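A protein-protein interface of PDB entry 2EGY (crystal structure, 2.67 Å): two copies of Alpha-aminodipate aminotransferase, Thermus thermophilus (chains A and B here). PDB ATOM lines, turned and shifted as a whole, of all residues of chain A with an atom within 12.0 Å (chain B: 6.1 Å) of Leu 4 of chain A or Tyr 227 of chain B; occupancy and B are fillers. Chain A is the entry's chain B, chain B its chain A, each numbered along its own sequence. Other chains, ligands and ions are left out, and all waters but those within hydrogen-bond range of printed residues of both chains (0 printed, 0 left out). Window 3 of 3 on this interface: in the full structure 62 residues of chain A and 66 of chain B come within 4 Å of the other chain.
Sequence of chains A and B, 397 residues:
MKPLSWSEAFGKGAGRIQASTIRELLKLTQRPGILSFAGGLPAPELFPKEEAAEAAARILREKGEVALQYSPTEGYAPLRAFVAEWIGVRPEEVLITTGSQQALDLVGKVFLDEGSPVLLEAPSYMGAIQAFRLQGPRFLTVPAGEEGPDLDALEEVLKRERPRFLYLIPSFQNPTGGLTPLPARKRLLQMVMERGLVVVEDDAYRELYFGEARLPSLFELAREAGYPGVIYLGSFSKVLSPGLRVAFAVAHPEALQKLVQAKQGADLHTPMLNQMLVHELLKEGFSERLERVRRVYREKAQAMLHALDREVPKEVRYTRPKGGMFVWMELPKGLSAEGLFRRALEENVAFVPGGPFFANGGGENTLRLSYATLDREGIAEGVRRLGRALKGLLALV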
ATOM      1  N   LYS A   2      -2.216  10.307 -26.769  1.00  0.00           N
ATOM      2  CA  LYS A   2      -1.021  10.950 -27.393  1.00  0.00           C
ATOM      3  C   LYS A   2      -1.158  12.475 -27.515  1.00  0.00           C
ATOM      4  O   LYS A   2      -2.265  13.017 -27.418  1.00  0.00           O
ATOM      5  CB  LYS A   2      -0.750  10.322 -28.763  1.00  0.00           C
ATOM      6  CG  LYS A   2       0.074   9.033 -28.714  1.00  0.00           C
ATOM      7  CD  LYS A   2       1.527   9.291 -28.289  1.00  0.00           C
ATOM      8  CE  LYS A   2       1.785   8.971 -26.816  1.00  0.00           C
ATOM      9  NZ  LYS A   2       1.054   9.846 -25.857  1.00  0.00           N
ATOM     10  N   PRO A   3      -0.026  13.183 -27.746  1.00  0.00           N
ATOM     11  CA  PRO A   3       0.004  14.646 -27.874  1.00  0.00           C
ATOM     12  C   PRO A   3      -1.034  15.267 -28.802  1.00  0.00           C
ATOM     13  O   PRO A   3      -1.779  14.568 -29.497  1.00  0.00           O
ATOM     14  CB  PRO A   3       1.443  14.930 -28.318  1.00  0.00           C
ATOM     15  CG  PRO A   3       1.825  13.695 -29.044  1.00  0.00           C
ATOM     16  CD  PRO A   3       1.277  12.619 -28.142  1.00  0.00           C
ATOM     17  N   LEU A   4      -1.080  16.594 -28.797  1.00  0.00           N
ATOM     18  CA  LEU A   4      -2.025  17.330 -29.618  1.00  0.00           C
ATOM     19  C   LEU A   4      -1.367  17.934 -30.847  1.00  0.00           C
ATOM     20  O   LEU A   4      -0.386  18.671 -30.741  1.00  0.00           O
ATOM     21  CB  LEU A   4      -2.669  18.460 -28.807  1.00  0.00           C
ATOM     22  CG  LEU A   4      -4.193  18.481 -28.764  1.00  0.00           C
ATOM     23  CD1 LEU A   4      -4.654  17.344 -27.888  1.00  0.00           C
ATOM     24  CD2 LEU A   4      -4.695  19.795 -28.216  1.00  0.00           C
ATOM     25  N   SER A   5      -1.905  17.608 -32.015  1.00  0.00           N
ATOM     26  CA  SER A   5      -1.396  18.164 -33.254  1.00  0.00           C
ATOM     27  C   SER A   5      -2.538  19.021 -33.754  1.00  0.00           C
ATOM     28  O   SER A   5      -3.472  18.535 -34.390  1.00  0.00           O
ATOM     29  CB  SER A   5      -1.076  17.069 -34.273  1.00  0.00           C
ATOM     30  OG  SER A   5      -0.591  17.632 -35.481  1.00  0.00           O
ATOM     31  N   TRP A   6      -2.479  20.299 -33.425  1.00  0.00           N
ATOM     32  CA  TRP A   6      -3.516  21.219 -33.840  1.00  0.00           C
ATOM     33  C   TRP A   6      -3.751  21.132 -35.338  1.00  0.00           C
ATOM     34  O   TRP A   6      -4.886  20.973 -35.786  1.00  0.00           O
ATOM     35  CB  TRP A   6      -3.125  22.641 -33.451  1.00  0.00           C
ATOM     36  CG  TRP A   6      -3.192  22.873 -31.982  1.00  0.00           C
ATOM     37  CD1 TRP A   6      -2.146  23.049 -31.125  1.00  0.00           C
ATOM     38  CD2 TRP A   6      -4.379  22.957 -31.194  1.00  0.00           C
ATOM     39  NE1 TRP A   6      -2.611  23.243 -29.848  1.00  0.00           N
ATOM     40  CE2 TRP A   6      -3.981  23.192 -29.864  1.00  0.00           C
ATOM     41  CE3 TRP A   6      -5.745  22.859 -31.486  1.00  0.00           C
ATOM     42  CZ2 TRP A   6      -4.901  23.333 -28.823  1.00  0.00           C
ATOM     43  CZ3 TRP A   6      -6.658  22.998 -30.455  1.00  0.00           C
ATOM     44  CH2 TRP A   6      -6.232  23.234 -29.138  1.00  0.00           C
ATOM     45  N   SER A   7      -2.664  21.226 -36.100  1.00  0.00           N
ATOM     46  CA  SER A   7      -2.708  21.178 -37.559  1.00  0.00           C
ATOM     47  C   SER A   7      -3.670  20.135 -38.124  1.00  0.00           C
ATOM     48  O   SER A   7      -4.153  20.279 -39.252  1.00  0.00           O
ATOM     49  CB  SER A   7      -1.303  20.928 -38.110  1.00  0.00           C
ATOM     50  OG  SER A   7      -0.421  21.969 -37.727  1.00  0.00           O
ATOM     51  N   GLU A   8      -3.948  19.094 -37.339  1.00  0.00           N
ATOM     52  CA  GLU A   8      -4.854  18.028 -37.761  1.00  0.00           C
ATOM     53  C   GLU A   8      -6.114  18.003 -36.903  1.00  0.00           C
ATOM     54  O   GLU A   8      -7.087  17.316 -37.229  1.00  0.00           O
ATOM     55  CB  GLU A   8      -4.163  16.665 -37.663  1.00  0.00           C
ATOM     56  CG  GLU A   8      -3.888  16.227 -36.243  1.00  0.00           C
ATOM     57  CD  GLU A   8      -4.346  14.811 -35.979  1.00  0.00           C
ATOM     58  OE1 GLU A   8      -3.737  13.874 -36.534  1.00  0.00           O
ATOM     59  OE2 GLU A   8      -5.323  14.636 -35.218  1.00  0.00           O
ATOM     60  N   ALA A   9      -6.084  18.740 -35.796  1.00  0.00           N
ATOM     61  CA  ALA A   9      -7.227  18.806 -34.893  1.00  0.00           C
ATOM     62  C   ALA A   9      -8.316  19.632 -35.560  1.00  0.00           C
ATOM     63  O   ALA A   9      -9.513  19.408 -35.349  1.00  0.00           O
ATOM     64  CB  ALA A   9      -6.811  19.452 -33.580  1.00  0.00           C
ATOM     65  N   PHE A  10      -7.875  20.584 -36.375  1.00  0.00           N
ATOM     66  CA  PHE A  10      -8.766  21.477 -37.093  1.00  0.00           C
ATOM     67  C   PHE A  10      -9.585  20.739 -38.132  1.00  0.00           C
ATOM     68  O   PHE A  10      -9.311  19.584 -38.446  1.00  0.00           O
ATOM     69  CB  PHE A  10      -7.963  22.562 -37.804  1.00  0.00           C
ATOM     70  CG  PHE A  10      -7.088  23.374 -36.899  1.00  0.00           C
ATOM     71  CD1 PHE A  10      -7.567  23.848 -35.682  1.00  0.00           C
ATOM     72  CD2 PHE A  10      -5.803  23.722 -37.295  1.00  0.00           C
ATOM     73  CE1 PHE A  10      -6.786  24.658 -34.877  1.00  0.00           C
ATOM     74  CE2 PHE A  10      -5.010  24.535 -36.496  1.00  0.00           C
ATOM     75  CZ  PHE A  10      -5.503  25.006 -35.282  1.00  0.00           C
ATOM     76  N   LEU B 189     -10.656  15.608 -17.276  1.00  0.00           N
ATOM     77  CA  LEU B 189      -9.413  16.040 -17.882  1.00  0.00           C
ATOM     78  C   LEU B 189      -8.536  14.818 -18.123  1.00  0.00           C
ATOM     79  O   LEU B 189      -7.881  14.711 -19.157  1.00  0.00           O
ATOM     80  CB  LEU B 189      -8.684  17.019 -16.970  1.00  0.00           C
ATOM     81  CG  LEU B 189      -7.252  17.333 -17.385  1.00  0.00           C
ATOM     82  CD1 LEU B 189      -7.246  17.918 -18.777  1.00  0.00           C
ATOM     83  CD2 LEU B 189      -6.637  18.296 -16.387  1.00  0.00           C
ATOM     84  N   VAL B 192      -9.574  13.339 -21.440  1.00  0.00           N
ATOM     85  CA  VAL B 192      -9.253  13.981 -22.710  1.00  0.00           C
ATOM     86  C   VAL B 192      -7.747  14.033 -22.932  1.00  0.00           C
ATOM     87  O   VAL B 192      -7.288  14.076 -24.064  1.00  0.00           O
ATOM     88  CB  VAL B 192      -9.860  15.419 -22.828  1.00  0.00           C
ATOM     89  CG1 VAL B 192     -11.323  15.400 -22.437  1.00  0.00           C
ATOM     90  CG2 VAL B 192      -9.089  16.397 -21.981  1.00  0.00           C
ATOM     91  N   MET B 193      -6.971  14.030 -21.856  1.00  0.00           N
ATOM     92  CA  MET B 193      -5.521  14.044 -21.995  1.00  0.00           C
ATOM     93  C   MET B 193      -5.052  12.681 -22.481  1.00  0.00           C
ATOM     94  O   MET B 193      -4.103  12.578 -23.252  1.00  0.00           O
ATOM     95  CB  MET B 193      -4.843  14.339 -20.664  1.00  0.00           C
ATOM     96  CG  MET B 193      -4.807  15.783 -20.281  1.00  0.00           C
ATOM     97  SD  MET B 193      -3.511  16.005 -19.084  1.00  0.00           S
ATOM     98  CE  MET B 193      -4.359  15.557 -17.600  1.00  0.00           C
ATOM     99  N   ARG B 195      -6.536  10.902 -24.429  1.00  0.00           N
ATOM    100  CA  ARG B 195      -6.897  10.781 -25.833  1.00  0.00           C
ATOM    101  C   ARG B 195      -6.599  11.998 -26.691  1.00  0.00           C
ATOM    102  O   ARG B 195      -7.135  12.113 -27.787  1.00  0.00           O
ATOM    103  CB  ARG B 195      -8.376  10.454 -25.932  1.00  0.00           C
ATOM    104  CG  ARG B 195      -8.661   9.164 -26.639  1.00  0.00           C
ATOM    105  CD  ARG B 195     -10.042   8.674 -26.278  1.00  0.00           C
ATOM    106  NE  ARG B 195     -10.195   8.602 -24.831  1.00  0.00           N
ATOM    107  CZ  ARG B 195     -10.819   7.612 -24.201  1.00  0.00           C
ATOM    108  NH1 ARG B 195     -11.340   6.609 -24.897  1.00  0.00           N
ATOM    109  NH2 ARG B 195     -10.928   7.633 -22.877  1.00  0.00           N
ATOM    110  N   GLY B 196      -5.748  12.894 -26.203  1.00  0.00           N
ATOM    111  CA  GLY B 196      -5.425  14.093 -26.956  1.00  0.00           C
ATOM    112  C   GLY B 196      -6.657  14.732 -27.586  1.00  0.00           C
ATOM    113  O   GLY B 196      -6.673  15.005 -28.792  1.00  0.00           O
ATOM    114  N   LEU B 197      -7.685  14.976 -26.770  1.00  0.00           N
ATOM    115  CA  LEU B 197      -8.943  15.567 -27.235  1.00  0.00           C
ATOM    116  C   LEU B 197      -9.077  17.052 -26.889  1.00  0.00           C
ATOM    117  O   LEU B 197      -8.450  17.545 -25.955  1.00  0.00           O
ATOM    118  CB  LEU B 197     -10.124  14.804 -26.633  1.00  0.00           C
ATOM    119  CG  LEU B 197     -10.232  13.321 -26.981  1.00  0.00           C
ATOM    120  CD1 LEU B 197     -11.300  12.668 -26.136  1.00  0.00           C
ATOM    121  CD2 LEU B 197     -10.559  13.176 -28.451  1.00  0.00           C
ATOM    122  N   VAL B 198      -9.902  17.763 -27.650  1.00  0.00           N
ATOM    123  CA  VAL B 198     -10.109  19.188 -27.407  1.00  0.00           C
ATOM    124  C   VAL B 198     -11.355  19.429 -26.555  1.00  0.00           C
ATOM    125  O   VAL B 198     -12.373  18.758 -26.713  1.00  0.00           O
ATOM    126  CB  VAL B 198     -10.241  19.982 -28.743  1.00  0.00           C
ATOM    127  CG1 VAL B 198     -10.530  21.455 -28.460  1.00  0.00           C
ATOM    128  CG2 VAL B 198      -8.951  19.855 -29.557  1.00  0.00           C
ATOM    129  N   VAL B 199     -11.250  20.383 -25.639  1.00  0.00           N
ATOM    130  CA  VAL B 199     -12.351  20.749 -24.761  1.00  0.00           C
ATOM    131  C   VAL B 199     -12.582  22.253 -24.789  1.00  0.00           C
ATOM    132  O   VAL B 199     -11.692  23.051 -24.478  1.00  0.00           O
ATOM    133  CB  VAL B 199     -12.081  20.345 -23.299  1.00  0.00           C
ATOM    134  CG1 VAL B 199     -13.049  21.072 -22.378  1.00  0.00           C
ATOM    135  CG2 VAL B 199     -12.247  18.849 -23.129  1.00  0.00           C
ATOM    136  N   PHE B 219      -9.473  24.673 -17.596  1.00  0.00           N
ATOM    137  CA  PHE B 219      -8.324  25.349 -18.194  1.00  0.00           C
ATOM    138  C   PHE B 219      -7.210  25.440 -17.160  1.00  0.00           C
ATOM    139  O   PHE B 219      -6.026  25.380 -17.495  1.00  0.00           O
ATOM    140  CB  PHE B 219      -8.685  26.763 -18.647  1.00  0.00           C
ATOM    141  CG  PHE B 219      -7.546  27.494 -19.315  1.00  0.00           C
ATOM    142  CD1 PHE B 219      -7.322  27.369 -20.685  1.00  0.00           C
ATOM    143  CD2 PHE B 219      -6.689  28.300 -18.575  1.00  0.00           C
ATOM    144  CE1 PHE B 219      -6.262  28.041 -21.304  1.00  0.00           C
ATOM    145  CE2 PHE B 219      -5.631  28.969 -19.189  1.00  0.00           C
ATOM    146  CZ  PHE B 219      -5.418  28.839 -20.555  1.00  0.00           C
ATOM    147  N   ALA B 222      -5.803  21.849 -16.458  1.00  0.00           N
ATOM    148  CA  ALA B 222      -5.032  21.469 -17.637  1.00  0.00           C
ATOM    149  C   ALA B 222      -3.692  22.189 -17.730  1.00  0.00           C
ATOM    150  O   ALA B 222      -2.647  21.548 -17.795  1.00  0.00           O
ATOM    151  CB  ALA B 222      -5.845  21.724 -18.894  1.00  0.00           C
ATOM    152  N   ARG B 223      -3.717  23.518 -17.754  1.00  0.00           N
ATOM    153  CA  ARG B 223      -2.476  24.278 -17.838  1.00  0.00           C
ATOM    154  C   ARG B 223      -1.476  23.768 -16.805  1.00  0.00           C
ATOM    155  O   ARG B 223      -0.281  23.664 -17.070  1.00  0.00           O
ATOM    156  CB  ARG B 223      -2.736  25.771 -17.609  1.00  0.00           C
ATOM    157  CG  ARG B 223      -1.483  26.551 -17.241  1.00  0.00           C
ATOM    158  CD  ARG B 223      -1.672  28.062 -17.275  1.00  0.00           C
ATOM    159  NE  ARG B 223      -1.545  28.597 -18.627  1.00  0.00           N
ATOM    160  CZ  ARG B 223      -0.912  29.729 -18.928  1.00  0.00           C
ATOM    161  NH1 ARG B 223      -0.851  30.136 -20.186  1.00  0.00           N
ATOM    162  NH2 ARG B 223      -0.330  30.449 -17.976  1.00  0.00           N
ATOM    163  N   GLU B 224      -1.981  23.444 -15.626  1.00  0.00           N
ATOM    164  CA  GLU B 224      -1.144  22.952 -14.555  1.00  0.00           C
ATOM    165  C   GLU B 224      -0.595  21.570 -14.906  1.00  0.00           C
ATOM    166  O   GLU B 224       0.525  21.218 -14.538  1.00  0.00           O
ATOM    167  CB  GLU B 224      -1.965  22.889 -13.273  1.00  0.00           C
ATOM    168  CG  GLU B 224      -1.166  22.582 -12.032  1.00  0.00           C
ATOM    169  CD  GLU B 224      -1.993  22.734 -10.772  1.00  0.00           C
ATOM    170  OE1 GLU B 224      -3.006  22.008 -10.631  1.00  0.00           O
ATOM    171  OE2 GLU B 224      -1.632  23.584  -9.925  1.00  0.00           O
ATOM    172  N   ALA B 225      -1.385  20.789 -15.629  1.00  0.00           N
ATOM    173  CA  ALA B 225      -0.962  19.453 -16.016  1.00  0.00           C
ATOM    174  C   ALA B 225      -0.025  19.494 -17.215  1.00  0.00           C
ATOM    175  O   ALA B 225       0.741  18.559 -17.436  1.00  0.00           O
ATOM    176  CB  ALA B 225      -2.173  18.592 -16.334  1.00  0.00           C
ATOM    177  N   GLY B 226      -0.091  20.578 -17.984  1.00  0.00           N
ATOM    178  CA  GLY B 226       0.758  20.718 -19.159  1.00  0.00           C
ATOM    179  C   GLY B 226       0.033  20.510 -20.481  1.00  0.00           C
ATOM    180  O   GLY B 226       0.567  20.811 -21.549  1.00  0.00           O
ATOM    181  N   TYR B 227      -1.188  19.995 -20.407  1.00  0.00           N
ATOM    182  CA  TYR B 227      -2.008  19.734 -21.587  1.00  0.00           C
ATOM    183  C   TYR B 227      -2.558  21.042 -22.154  1.00  0.00           C
ATOM    184  O   TYR B 227      -3.126  21.853 -21.426  1.00  0.00           O
ATOM    185  CB  TYR B 227      -3.165  18.808 -21.201  1.00  0.00           C
ATOM    186  CG  TYR B 227      -3.962  18.288 -22.365  1.00  0.00           C
ATOM    187  CD1 TYR B 227      -3.361  17.508 -23.346  1.00  0.00           C
ATOM    188  CD2 TYR B 227      -5.321  18.577 -22.486  1.00  0.00           C
ATOM    189  CE1 TYR B 227      -4.085  17.026 -24.420  1.00  0.00           C
ATOM    190  CE2 TYR B 227      -6.059  18.099 -23.558  1.00  0.00           C
ATOM    191  CZ  TYR B 227      -5.433  17.323 -24.523  1.00  0.00           C
ATOM    192  OH  TYR B 227      -6.152  16.842 -25.592  1.00  0.00           O
ATOM    193  N   PRO B 228      -2.389  21.266 -23.466  1.00  0.00           N
ATOM    194  CA  PRO B 228      -2.878  22.490 -24.110  1.00  0.00           C
ATOM    195  C   PRO B 228      -4.139  22.259 -24.948  1.00  0.00           C
ATOM    196  O   PRO B 228      -4.333  22.917 -25.965  1.00  0.00           O
ATOM    197  CB  PRO B 228      -1.704  22.875 -24.985  1.00  0.00           C
ATOM    198  CG  PRO B 228      -1.315  21.522 -25.536  1.00  0.00           C
ATOM    199  CD  PRO B 228      -1.390  20.600 -24.325  1.00  0.00           C
ATOM    200  N   GLY B 229      -4.995  21.335 -24.534  1.00  0.00           N
ATOM    201  CA  GLY B 229      -6.178  21.064 -25.328  1.00  0.00           C
ATOM    202  C   GLY B 229      -7.454  21.781 -24.936  1.00  0.00           C
ATOM    203  O   GLY B 229      -8.529  21.457 -25.447  1.00  0.00           O
ATOM    204  N   VAL B 230      -7.350  22.761 -24.045  1.00  0.00           N
ATOM    205  CA  VAL B 230      -8.535  23.474 -23.606  1.00  0.00           C
ATOM    206  C   VAL B 230      -8.646  24.891 -24.155  1.00  0.00           C
ATOM    207  O   VAL B 230      -7.688  25.667 -24.125  1.00  0.00           O
ATOM    208  CB  VAL B 230      -8.602  23.549 -22.067  1.00  0.00           C
ATOM    209  CG1 VAL B 230      -9.967  24.039 -21.644  1.00  0.00           C
ATOM    210  CG2 VAL B 230      -8.317  22.195 -21.455  1.00  0.00           C
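The backbone NH (N) of Val 199 of chain B sits at hydrogen-bond distance from the backbone carbonyl oxygen (O) of Gly 229 of chain B.
The backbone NH of Tyr 227 of chain B is in hydrogen-bond range of the backbone carbonyl oxygen of Ala 222 of chain B (3.4 Å).
The side-chain hydroxyl (OH) of Tyr 227 of chain B lies within hydrogen-bond range of the backbone carbonyl oxygen (O) of Val 192 of chain B (3.4 Å).
The side-chain hydroxyl (OH) of Tyr 227 of chain B is in hydrogen-bond range of the backbone carbonyl oxygen (O) of Leu 197 of chain B.
Among the printed residues, pairs that only touch across the chains: Lys 2 of chain A with Gly 196 of chain B, Leu 4 of chain A with Gly 196 of chain B, Leu 4 of chain A with Tyr 227 of chain B, Leu 4 of chain A with Pro 228 of chain B, Leu 4 of chain A with Gly 229 of chain B, Trp 6 of chain A with Val 198 of chain B and Trp 6 of chain A with Pro 228 of chain B.
Printed residues of chain B within 4 Å of Lys 2 of chain A: Gly 196.
Printed residues of chain B within 4 Å of Leu 4 of chain A: Gly 196 (3.2 Å), Tyr 227 (2.8 Å), Pro 228 (3.9 Å) and Gly 229 (3.5 Å).
Printed residues of chain B within 4 Å of Trp 6 of chain A: Val 198 and Pro 228.
No residue of chain A comes within 4 Å of Val 192 of chain B.
No residue of chain A comes within 4 Å of Met 193 of chain B.
Gly 196 of chain B touches just these residues of chain A: Lys 2 (3.4 Å) and Leu 4 (3.2 Å).
Leu 197 of chain B touches none of the printed residues of chain A.
Of the printed residues of chain A, Val 198 of chain B touches Trp 6.
No residue of chain A comes within 4 Å of Phe 219 of chain B.
Arg 223 of chain B touches none of the printed residues of chain A.
No residue of chain A comes within 4 Å of Gly 226 of chain B.
Tyr 227 of chain B touches just one residue of chain A: Leu 4 (2.8 Å).
Pro 228 of chain B touches just these residues of chain A: Leu 4 (3.9 Å) and Trp 6 (2.9 Å).
The nearest printed residue of chain B that does not touch Leu 4 of chain A is Leu 197 of chain B (4.01 Å).
The nearest residue of chain A that does not touch Tyr 227 of chain B is Lys 2 of chain A (5.3 Å).
Of the 18 printed residues of chain B, 5 touch a printed residue of chain A.
Among the printed residues, no Asp or Glu carboxylate lies within 4 Å of a Lys or Arg side-chain nitrogen of the other chain.
No position is printed for both chains.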
